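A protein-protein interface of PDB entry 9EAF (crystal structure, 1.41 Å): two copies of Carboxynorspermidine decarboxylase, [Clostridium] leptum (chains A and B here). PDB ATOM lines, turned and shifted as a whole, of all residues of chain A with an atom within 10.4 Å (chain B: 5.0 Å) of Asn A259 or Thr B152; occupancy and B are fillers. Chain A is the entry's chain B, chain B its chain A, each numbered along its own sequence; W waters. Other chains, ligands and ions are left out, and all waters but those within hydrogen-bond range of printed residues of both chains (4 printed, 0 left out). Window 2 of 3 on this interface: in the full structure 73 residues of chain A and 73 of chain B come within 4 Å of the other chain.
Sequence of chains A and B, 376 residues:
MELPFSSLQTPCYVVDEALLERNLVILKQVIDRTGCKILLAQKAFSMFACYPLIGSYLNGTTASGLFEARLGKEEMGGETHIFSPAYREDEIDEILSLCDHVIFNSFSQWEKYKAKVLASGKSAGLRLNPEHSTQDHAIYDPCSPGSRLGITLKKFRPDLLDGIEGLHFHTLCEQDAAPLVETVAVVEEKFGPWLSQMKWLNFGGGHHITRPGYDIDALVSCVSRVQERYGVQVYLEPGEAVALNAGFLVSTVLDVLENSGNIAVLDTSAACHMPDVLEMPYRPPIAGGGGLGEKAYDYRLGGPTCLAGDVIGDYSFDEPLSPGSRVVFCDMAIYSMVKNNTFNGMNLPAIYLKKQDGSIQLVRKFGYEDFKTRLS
OD1 of Asn B129 lies within hydrogen-bond range of N of Glu B131, 2.8 Å away.
The backbone carbonyl oxygen (O) of Ile B151 sits at hydrogen-bond distance from the backbone NH (N) of Asn B129 (2.8 Å).
The side-chain carboxylate of Glu A258 lies within hydrogen-bond range of the backbone NH of Gly A261, at 3.0 Å.
OE2 of Glu A258 is in hydrogen-bond range of N of Ser A260 (3.3 Å).
The backbone carbonyl oxygen (O) of Leu A257 is in hydrogen-bond range of the backbone NH (N) of Ile A263, 2.8 Å away.
Among the printed residues, merely in contact across the chains: Asn A259 with Gly B146 (3.3 Å), Ile A263 with Gly B146 (3.3 Å), Ile A263 with Ser B147 (3.8 Å), Asn A259 with Thr B152 (3.8 Å) and Asn A259 with Asn B129 (3.9 Å).
Along chain B the printed residues that touch a printed residue of chain A span positions 129 to 155.
Hydrophobic or aromatic side chains of chain A that line the printed part of chain B: Ile A263.
Water W2 lies within hydrogen-bond range of the backbone carbonyl oxygen (O) of Gly B150 (2.7 Å), the backbone carbonyl oxygen (O) of Ser B147 (2.9 Å), the side-chain amide nitrogen (ND2) of Asn B129 (3.1 Å) and the side-chain amide nitrogen (ND2) of Asn A259 (3.2 Å).
Water W1 lies within hydrogen-bond range of the side-chain amide oxygen of Asn A259 (2.7 Å), the side-chain hydroxyl of Ser A260 (2.7 Å) and the backbone NH of Gly B146 (3.0 Å).
Water W3 lies within hydrogen-bond range of the backbone carbonyl oxygen of Ser B144 (2.8 Å), the side-chain amide nitrogen of Asn B129 (2.9 Å) and the side-chain amide nitrogen of Asn A259 (3.0 Å).
Water W4 bridges the side-chain amide oxygen (OD1) of Asn A259 (2.8 Å) and the side-chain hydroxyl (OG1) of Thr B152 (2.9 Å).
OE1 of Glu A258 lies within salt-bridge range of NZ of Lys B155 (2.8 Å).
ND2 of Asn A259 lies within hydrogen-bond range of O of Ser B147 (2.9 Å).
Of chain B, only Asn B129 (3.9 Å), Gly B146 (3.3 Å), Ser B147 (2.9 Å) and Thr B152 (3.8 Å) come within 4 Å of Asn A259.
Of chain A, only Asn A259 (3.8 Å) comes within 4 Å of Thr B152.
Asn B129 touches just one residue of chain A: Asn A259.
Of chain A, only Asn A259 and Ile A263 come within 4 Å of Gly B146.
Of chain A, only Asn A259 (2.9 Å) and Ile A263 (3.8 Å) come within 4 Å of Ser B147.
No residue of chain A comes within 4 Å of Ile B151.
No residue of chain A comes within 4 Å of Leu B153.
Lys B155 touches one residue of chain A.
Of the printed residues of chain B, Ile A263 touches Gly B146 and Ser B147.
Of the printed residues of chain B, Glu A258 touches Lys B155 (2.8 Å).
Gly A261 touches none of the printed residues of chain B.
Ser B144 touches none of the printed residues of chain A.
The nearest printed residue of chain B that does not touch Glu A258 is Lys B154 (4.9 Å).
No position is printed for both chains.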
ATOM      1  N   VAL A 256     -15.728  19.011  30.274  1.00  0.00           N
ATOM      2  CA  VAL A 256     -16.666  20.093  30.538  1.00  0.00           C
ATOM      3  C   VAL A 256     -15.877  21.253  31.125  1.00  0.00           C
ATOM      4  O   VAL A 256     -15.038  21.056  32.009  1.00  0.00           O
ATOM      5  CB  VAL A 256     -17.801  19.667  31.491  1.00  0.00           C
ATOM      6  CG1 VAL A 256     -18.736  20.845  31.780  1.00  0.00           C
ATOM      7  CG2 VAL A 256     -18.589  18.513  30.895  1.00  0.00           C
ATOM      8  N   LEU A 257     -16.132  22.454  30.623  1.00  0.00           N
ATOM      9  CA  LEU A 257     -15.432  23.637  31.095  1.00  0.00           C
ATOM     10  C   LEU A 257     -16.417  24.792  31.170  1.00  0.00           C
ATOM     11  O   LEU A 257     -17.562  24.693  30.725  1.00  0.00           O
ATOM     12  CB  LEU A 257     -14.211  23.956  30.222  1.00  0.00           C
ATOM     13  CG  LEU A 257     -14.479  24.261  28.750  1.00  0.00           C
ATOM     14  CD1 LEU A 257     -14.294  25.745  28.499  1.00  0.00           C
ATOM     15  CD2 LEU A 257     -13.566  23.443  27.841  1.00  0.00           C
ATOM     16  N   GLU A 258     -15.972  25.885  31.779  1.00  0.00           N
ATOM     17  CA  GLU A 258     -16.811  27.052  32.006  1.00  0.00           C
ATOM     18  C   GLU A 258     -16.181  28.254  31.322  1.00  0.00           C
ATOM     19  O   GLU A 258     -14.997  28.541  31.529  1.00  0.00           O
ATOM     20  CB  GLU A 258     -16.971  27.321  33.505  1.00  0.00           C
ATOM     21  CG  GLU A 258     -18.171  28.182  33.858  1.00  0.00           C
ATOM     22  CD  GLU A 258     -17.924  29.663  33.673  1.00  0.00           C
ATOM     23  OE1 GLU A 258     -16.803  30.125  33.966  1.00  0.00           O
ATOM     24  OE2 GLU A 258     -18.864  30.366  33.242  1.00  0.00           O
ATOM     25  N   ASN A 259     -16.968  28.939  30.491  1.00  0.00           N
ATOM     26  CA  ASN A 259     -16.526  30.192  29.882  1.00  0.00           C
ATOM     27  C   ASN A 259     -17.796  30.949  29.497  1.00  0.00           C
ATOM     28  O   ASN A 259     -18.363  30.704  28.429  1.00  0.00           O
ATOM     29  CB  ASN A 259     -15.639  29.939  28.676  1.00  0.00           C
ATOM     30  CG  ASN A 259     -15.117  31.221  28.068  1.00  0.00           C
ATOM     31  OD1 ASN A 259     -15.032  32.244  28.741  1.00  0.00           O
ATOM     32  ND2 ASN A 259     -14.780  31.179  26.788  1.00  0.00           N
ATOM     33  N   SER A 260     -18.237  31.848  30.376  1.00  0.00           N
ATOM     34  CA  SER A 260     -19.524  32.518  30.204  1.00  0.00           C
ATOM     35  C   SER A 260     -20.640  31.496  30.003  1.00  0.00           C
ATOM     36  O   SER A 260     -21.520  31.664  29.154  1.00  0.00           O
ATOM     37  CB  SER A 260     -19.481  33.519  29.048  1.00  0.00           C
ATOM     38  OG  SER A 260     -18.521  34.529  29.294  1.00  0.00           O
ATOM     39  N   GLY A 261     -20.597  30.425  30.787  1.00  0.00           N
ATOM     40  CA  GLY A 261     -21.554  29.340  30.692  1.00  0.00           C
ATOM     41  C   GLY A 261     -20.871  27.986  30.646  1.00  0.00           C
ATOM     42  O   GLY A 261     -19.655  27.869  30.517  1.00  0.00           O
ATOM     43  N   ASN A 262     -21.697  26.947  30.748  1.00  0.00           N
ATOM     44  CA  ASN A 262     -21.191  25.583  30.708  1.00  0.00           C
ATOM     45  C   ASN A 262     -20.960  25.149  29.269  1.00  0.00           C
ATOM     46  O   ASN A 262     -21.809  25.351  28.397  1.00  0.00           O
ATOM     47  CB  ASN A 262     -22.193  24.610  31.324  1.00  0.00           C
ATOM     48  CG  ASN A 262     -22.654  25.028  32.700  1.00  0.00           C
ATOM     49  OD1 ASN A 262     -21.855  25.415  33.552  1.00  0.00           O
ATOM     50  ND2 ASN A 262     -23.955  24.939  32.927  1.00  0.00           N
ATOM     51  N   ILE A 263     -19.815  24.517  29.035  1.00  0.00           N
ATOM     52  CA  ILE A 263     -19.437  24.006  27.727  1.00  0.00           C
ATOM     53  C   ILE A 263     -19.100  22.532  27.886  1.00  0.00           C
ATOM     54  O   ILE A 263     -18.404  22.153  28.833  1.00  0.00           O
ATOM     55  CB  ILE A 263     -18.227  24.773  27.169  1.00  0.00           C
ATOM     56  CG1 ILE A 263     -18.600  26.235  26.939  1.00  0.00           C
ATOM     57  CG2 ILE A 263     -17.736  24.124  25.886  1.00  0.00           C
ATOM     58  CD1 ILE A 263     -17.424  27.168  26.990  1.00  0.00           C
ATOM     59  N   ALA A 264     -19.601  21.701  26.979  1.00  0.00           N
ATOM     60  CA  ALA A 264     -19.228  20.296  26.933  1.00  0.00           C
ATOM     61  C   ALA A 264     -18.559  20.012  25.599  1.00  0.00           C
ATOM     62  O   ALA A 264     -19.108  20.346  24.543  1.00  0.00           O
ATOM     63  CB  ALA A 264     -20.445  19.385  27.104  1.00  0.00           C
ATOM     64  N   VAL A 265     -17.381  19.401  25.654  1.00  0.00           N
ATOM     65  CA  VAL A 265     -16.684  18.934  24.462  1.00  0.00           C
ATOM     66  C   VAL A 265     -17.048  17.469  24.261  1.00  0.00           C
ATOM     67  O   VAL A 265     -16.753  16.624  25.116  1.00  0.00           O
ATOM     68  CB  VAL A 265     -15.165  19.113  24.605  1.00  0.00           C
ATOM     69  CG1 VAL A 265     -14.445  18.586  23.367  1.00  0.00           C
ATOM     70  CG2 VAL A 265     -14.818  20.579  24.851  1.00  0.00           C
ATOM     71  N   ASP A 298     -27.920  24.585  31.329  1.00  0.00           N
ATOM     72  CA  ASP A 298     -27.685  24.932  29.935  1.00  0.00           C
ATOM     73  C   ASP A 298     -26.247  24.595  29.554  1.00  0.00           C
ATOM     74  O   ASP A 298     -25.312  24.904  30.297  1.00  0.00           O
ATOM     75  CB  ASP A 298     -27.904  26.428  29.706  1.00  0.00           C
ATOM     76  CG  ASP A 298     -29.363  26.832  29.777  1.00  0.00           C
ATOM     77  OD1 ASP A 298     -30.246  25.964  29.613  1.00  0.00           O
ATOM     78  OD2 ASP A 298     -29.625  28.037  29.979  1.00  0.00           O
ATOM     79  N   TYR A 299     -26.075  23.979  28.384  1.00  0.00           N
ATOM     80  CA  TYR A 299     -24.756  23.672  27.849  1.00  0.00           C
ATOM     81  C   TYR A 299     -24.670  24.081  26.388  1.00  0.00           C
ATOM     82  O   TYR A 299     -25.629  23.922  25.629  1.00  0.00           O
ATOM     83  CB  TYR A 299     -24.452  22.172  27.894  1.00  0.00           C
ATOM     84  CG  TYR A 299     -24.221  21.622  29.274  1.00  0.00           C
ATOM     85  CD1 TYR A 299     -25.275  21.133  30.033  1.00  0.00           C
ATOM     86  CD2 TYR A 299     -22.945  21.589  29.823  1.00  0.00           C
ATOM     87  CE1 TYR A 299     -25.067  20.624  31.295  1.00  0.00           C
ATOM     88  CE2 TYR A 299     -22.725  21.085  31.080  1.00  0.00           C
ATOM     89  CZ  TYR A 299     -23.789  20.606  31.819  1.00  0.00           C
ATOM     90  OH  TYR A 299     -23.573  20.102  33.080  1.00  0.00           O
ATOM     91  N   ARG A 300     -23.507  24.577  25.995  1.00  0.00           N
ATOM     92  CA  ARG A 300     -23.131  24.649  24.593  1.00  0.00           C
ATOM     93  C   ARG A 300     -22.290  23.416  24.287  1.00  0.00           C
ATOM     94  O   ARG A 300     -21.277  23.173  24.951  1.00  0.00           O
ATOM     95  CB  ARG A 300     -22.345  25.926  24.308  1.00  0.00           C
ATOM     96  CG  ARG A 300     -21.783  25.996  22.904  1.00  0.00           C
ATOM     97  CD  ARG A 300     -21.611  27.437  22.462  1.00  0.00           C
ATOM     98  NE  ARG A 300     -22.868  28.009  21.998  1.00  0.00           N
ATOM     99  CZ  ARG A 300     -23.103  29.307  21.857  1.00  0.00           C
ATOM    100  NH1 ARG A 300     -22.202  30.216  22.199  1.00  0.00           N
ATOM    101  NH2 ARG A 300     -24.271  29.704  21.362  1.00  0.00           N
ATOM    102  N   ASP A 314     -26.943  24.557  21.523  1.00  0.00           N
ATOM    103  CA  ASP A 314     -27.186  24.856  22.928  1.00  0.00           C
ATOM    104  C   ASP A 314     -28.382  24.044  23.404  1.00  0.00           C
ATOM    105  O   ASP A 314     -29.462  24.121  22.808  1.00  0.00           O
ATOM    106  CB  ASP A 314     -27.470  26.349  23.111  1.00  0.00           C
ATOM    107  CG  ASP A 314     -26.283  27.214  22.748  1.00  0.00           C
ATOM    108  OD1 ASP A 314     -25.141  26.769  22.972  1.00  0.00           O
ATOM    109  OD2 ASP A 314     -26.486  28.337  22.238  1.00  0.00           O
ATOM    110  N   ASN B 129      -6.622  31.347  25.893  1.00  0.00           N
ATOM    111  CA  ASN B 129      -7.618  32.173  25.222  1.00  0.00           C
ATOM    112  C   ASN B 129      -7.415  33.588  25.740  1.00  0.00           C
ATOM    113  O   ASN B 129      -7.873  33.911  26.849  1.00  0.00           O
ATOM    114  CB  ASN B 129      -9.030  31.683  25.554  1.00  0.00           C
ATOM    115  CG  ASN B 129     -10.110  32.552  24.940  1.00  0.00           C
ATOM    116  OD1 ASN B 129      -9.832  33.612  24.378  1.00  0.00           O
ATOM    117  ND2 ASN B 129     -11.357  32.112  25.061  1.00  0.00           N
ATOM    118  N   GLU B 131      -8.840  36.220  24.944  1.00  0.00           N
ATOM    119  CA  GLU B 131     -10.073  36.999  24.870  1.00  0.00           C
ATOM    120  C   GLU B 131      -9.830  38.341  24.192  1.00  0.00           C
ATOM    121  O   GLU B 131     -10.295  39.389  24.649  1.00  0.00           O
ATOM    122  CB  GLU B 131     -10.701  37.188  26.250  1.00  0.00           C
ATOM    123  CG  GLU B 131     -11.065  35.892  26.948  1.00  0.00           C
ATOM    124  CD  GLU B 131     -11.537  36.118  28.369  1.00  0.00           C
ATOM    125  OE1 GLU B 131     -10.684  36.387  29.239  1.00  0.00           O
ATOM    126  OE2 GLU B 131     -12.761  36.043  28.611  1.00  0.00           O
ATOM    127  N   SER B 144     -14.154  34.693  20.747  1.00  0.00           N
ATOM    128  CA  SER B 144     -15.508  35.148  21.011  1.00  0.00           C
ATOM    129  C   SER B 144     -15.961  34.651  22.381  1.00  0.00           C
ATOM    130  O   SER B 144     -15.495  33.613  22.860  1.00  0.00           O
ATOM    131  CB  SER B 144     -16.462  34.609  19.950  1.00  0.00           C
ATOM    132  OG  SER B 144     -16.327  35.321  18.738  1.00  0.00           O
ATOM    133  N   PRO B 145     -16.874  35.369  23.032  1.00  0.00           N
ATOM    134  CA  PRO B 145     -17.401  34.889  24.313  1.00  0.00           C
ATOM    135  C   PRO B 145     -17.958  33.481  24.171  1.00  0.00           C
ATOM    136  O   PRO B 145     -18.607  33.146  23.179  1.00  0.00           O
ATOM    137  CB  PRO B 145     -18.508  35.896  24.640  1.00  0.00           C
ATOM    138  CG  PRO B 145     -18.135  37.130  23.897  1.00  0.00           C
ATOM    139  CD  PRO B 145     -17.434  36.677  22.653  1.00  0.00           C
ATOM    140  N   GLY B 146     -17.683  32.645  25.170  1.00  0.00           N
ATOM    141  CA  GLY B 146     -18.170  31.282  25.178  1.00  0.00           C
ATOM    142  C   GLY B 146     -17.340  30.289  24.391  1.00  0.00           C
ATOM    143  O   GLY B 146     -17.734  29.120  24.298  1.00  0.00           O
ATOM    144  N   SER B 147     -16.210  30.708  23.826  1.00  0.00           N
ATOM    145  CA  SER B 147     -15.354  29.794  23.084  1.00  0.00           C
ATOM    146  C   SER B 147     -14.887  28.642  23.965  1.00  0.00           C
ATOM    147  O   SER B 147     -14.533  28.833  25.133  1.00  0.00           O
ATOM    148  CB  SER B 147     -14.128  30.544  22.574  1.00  0.00           C
ATOM    149  OG  SER B 147     -13.183  29.638  22.039  1.00  0.00           O
ATOM    150  N   GLY B 150      -9.010  27.044  24.489  1.00  0.00           N
ATOM    151  CA  GLY B 150      -8.032  27.758  25.279  1.00  0.00           C
ATOM    152  C   GLY B 150      -8.551  28.155  26.651  1.00  0.00           C
ATOM    153  O   GLY B 150      -9.749  28.171  26.923  1.00  0.00           O
ATOM    154  N   ILE B 151      -7.607  28.499  27.521  1.00  0.00           N
ATOM    155  CA  ILE B 151      -7.873  28.833  28.916  1.00  0.00           C
ATOM    156  C   ILE B 151      -7.876  30.347  29.059  1.00  0.00           C
ATOM    157  O   ILE B 151      -6.896  31.014  28.697  1.00  0.00           O
ATOM    158  CB  ILE B 151      -6.797  28.221  29.825  1.00  0.00           C
ATOM    159  CG1 ILE B 151      -6.789  26.698  29.701  1.00  0.00           C
ATOM    160  CG2 ILE B 151      -7.011  28.651  31.262  1.00  0.00           C
ATOM    161  CD1 ILE B 151      -5.429  26.090  29.967  1.00  0.00           C
ATOM    162  N   THR B 152      -8.963  30.891  29.598  1.00  0.00           N
ATOM    163  CA  THR B 152      -9.046  32.318  29.861  1.00  0.00           C
ATOM    164  C   THR B 152      -8.301  32.659  31.149  1.00  0.00           C
ATOM    165  O   THR B 152      -8.079  31.808  32.015  1.00  0.00           O
ATOM    166  CB  THR B 152     -10.508  32.763  29.982  1.00  0.00           C
ATOM    167  OG1 THR B 152     -11.177  31.979  30.982  1.00  0.00           O
ATOM    168  CG2 THR B 152     -11.232  32.611  28.656  1.00  0.00           C
ATOM    169  N   LEU B 153      -7.914  33.933  31.268  1.00  0.00           N
ATOM    170  CA  LEU B 153      -7.167  34.369  32.444  1.00  0.00           C
ATOM    171  C   LEU B 153      -7.913  34.037  33.733  1.00  0.00           C
ATOM    172  O   LEU B 153      -7.311  33.566  34.704  1.00  0.00           O
ATOM    173  CB  LEU B 153      -6.903  35.872  32.361  1.00  0.00           C
ATOM    174  CG  LEU B 153      -6.139  36.468  33.548  1.00  0.00           C
ATOM    175  CD1 LEU B 153      -4.794  35.788  33.707  1.00  0.00           C
ATOM    176  CD2 LEU B 153      -5.965  37.967  33.382  1.00  0.00           C
ATOM    177  N   LYS B 154      -9.226  34.283  33.760  1.00  0.00           N
ATOM    178  CA  LYS B 154     -10.017  34.027  34.959  1.00  0.00           C
ATOM    179  C   LYS B 154      -9.928  32.569  35.395  1.00  0.00           C
ATOM    180  O   LYS B 154     -10.106  32.265  36.581  1.00  0.00           O
ATOM    181  CB  LYS B 154     -11.469  34.418  34.672  1.00  0.00           C
ATOM    182  CG  LYS B 154     -12.433  34.282  35.837  1.00  0.00           C
ATOM    183  CD  LYS B 154     -13.776  33.726  35.372  1.00  0.00           C
ATOM    184  CE  LYS B 154     -14.616  34.779  34.661  1.00  0.00           C
ATOM    185  NZ  LYS B 154     -15.464  35.559  35.610  1.00  0.00           N
ATOM    186  N   LYS B 155      -9.648  31.660  34.462  1.00  0.00           N
ATOM    187  CA  LYS B 155      -9.568  30.233  34.740  1.00  0.00           C
ATOM    188  C   LYS B 155      -8.137  29.737  34.870  1.00  0.00           C
ATOM    189  O   LYS B 155      -7.924  28.536  35.069  1.00  0.00           O
ATOM    190  CB  LYS B 155     -10.266  29.447  33.626  1.00  0.00           C
ATOM    191  CG  LYS B 155     -11.725  29.789  33.461  1.00  0.00           C
ATOM    192  CD  LYS B 155     -12.513  29.465  34.716  1.00  0.00           C
ATOM    193  CE  LYS B 155     -13.978  29.710  34.492  1.00  0.00           C
ATOM    194  NZ  LYS B 155     -14.757  29.596  35.751  1.00  0.00           N
ATOM    195  N   PHE B 156      -7.157  30.624  34.768  1.00  0.00           N
ATOM    196  CA  PHE B 156      -5.764  30.212  34.748  1.00  0.00           C
ATOM    197  C   PHE B 156      -5.300  29.859  36.155  1.00  0.00           C
ATOM    198  O   PHE B 156      -5.639  30.538  37.128  1.00  0.00           O
ATOM    199  CB  PHE B 156      -4.913  31.338  34.166  1.00  0.00           C
ATOM    200  CG  PHE B 156      -3.551  30.903  33.733  1.00  0.00           C
ATOM    201  CD1 PHE B 156      -3.393  30.060  32.649  1.00  0.00           C
ATOM    202  CD2 PHE B 156      -2.423  31.350  34.394  1.00  0.00           C
ATOM    203  CE1 PHE B 156      -2.138  29.661  32.242  1.00  0.00           C
ATOM    204  CE2 PHE B 156      -1.165  30.953  33.988  1.00  0.00           C
ATOM    205  CZ  PHE B 156      -1.024  30.107  32.913  1.00  0.00           C
ATOM    206  N   PHE B 191      -0.966  37.309  30.736  1.00  0.00           N
ATOM    207  CA  PHE B 191      -0.230  36.120  31.147  1.00  0.00           C
ATOM    208  C   PHE B 191       1.259  36.379  31.335  1.00  0.00           C
ATOM    209  O   PHE B 191       2.016  35.432  31.573  1.00  0.00           O
ATOM    210  CB  PHE B 191      -0.455  34.999  30.129  1.00  0.00           C
ATOM    211  CG  PHE B 191      -1.900  34.619  29.962  1.00  0.00           C
ATOM    212  CD1 PHE B 191      -2.512  33.752  30.849  1.00  0.00           C
ATOM    213  CD2 PHE B 191      -2.649  35.142  28.919  1.00  0.00           C
ATOM    214  CE1 PHE B 191      -3.838  33.408  30.694  1.00  0.00           C
ATOM    215  CE2 PHE B 191      -3.978  34.802  28.761  1.00  0.00           C
ATOM    216  CZ  PHE B 191      -4.572  33.936  29.649  1.00  0.00           C
HETATM  217  O   HOH W   1     -16.511  34.134  27.514  1.00  0.00           O
HETATM  218  O   HOH W   2     -12.033  29.475  26.499  1.00  0.00           O
HETATM  219  O   HOH W   3     -13.897  33.494  25.112  1.00  0.00           O
HETATM  220  O   HOH W   4     -13.876  32.938  31.184  1.00  0.00           O
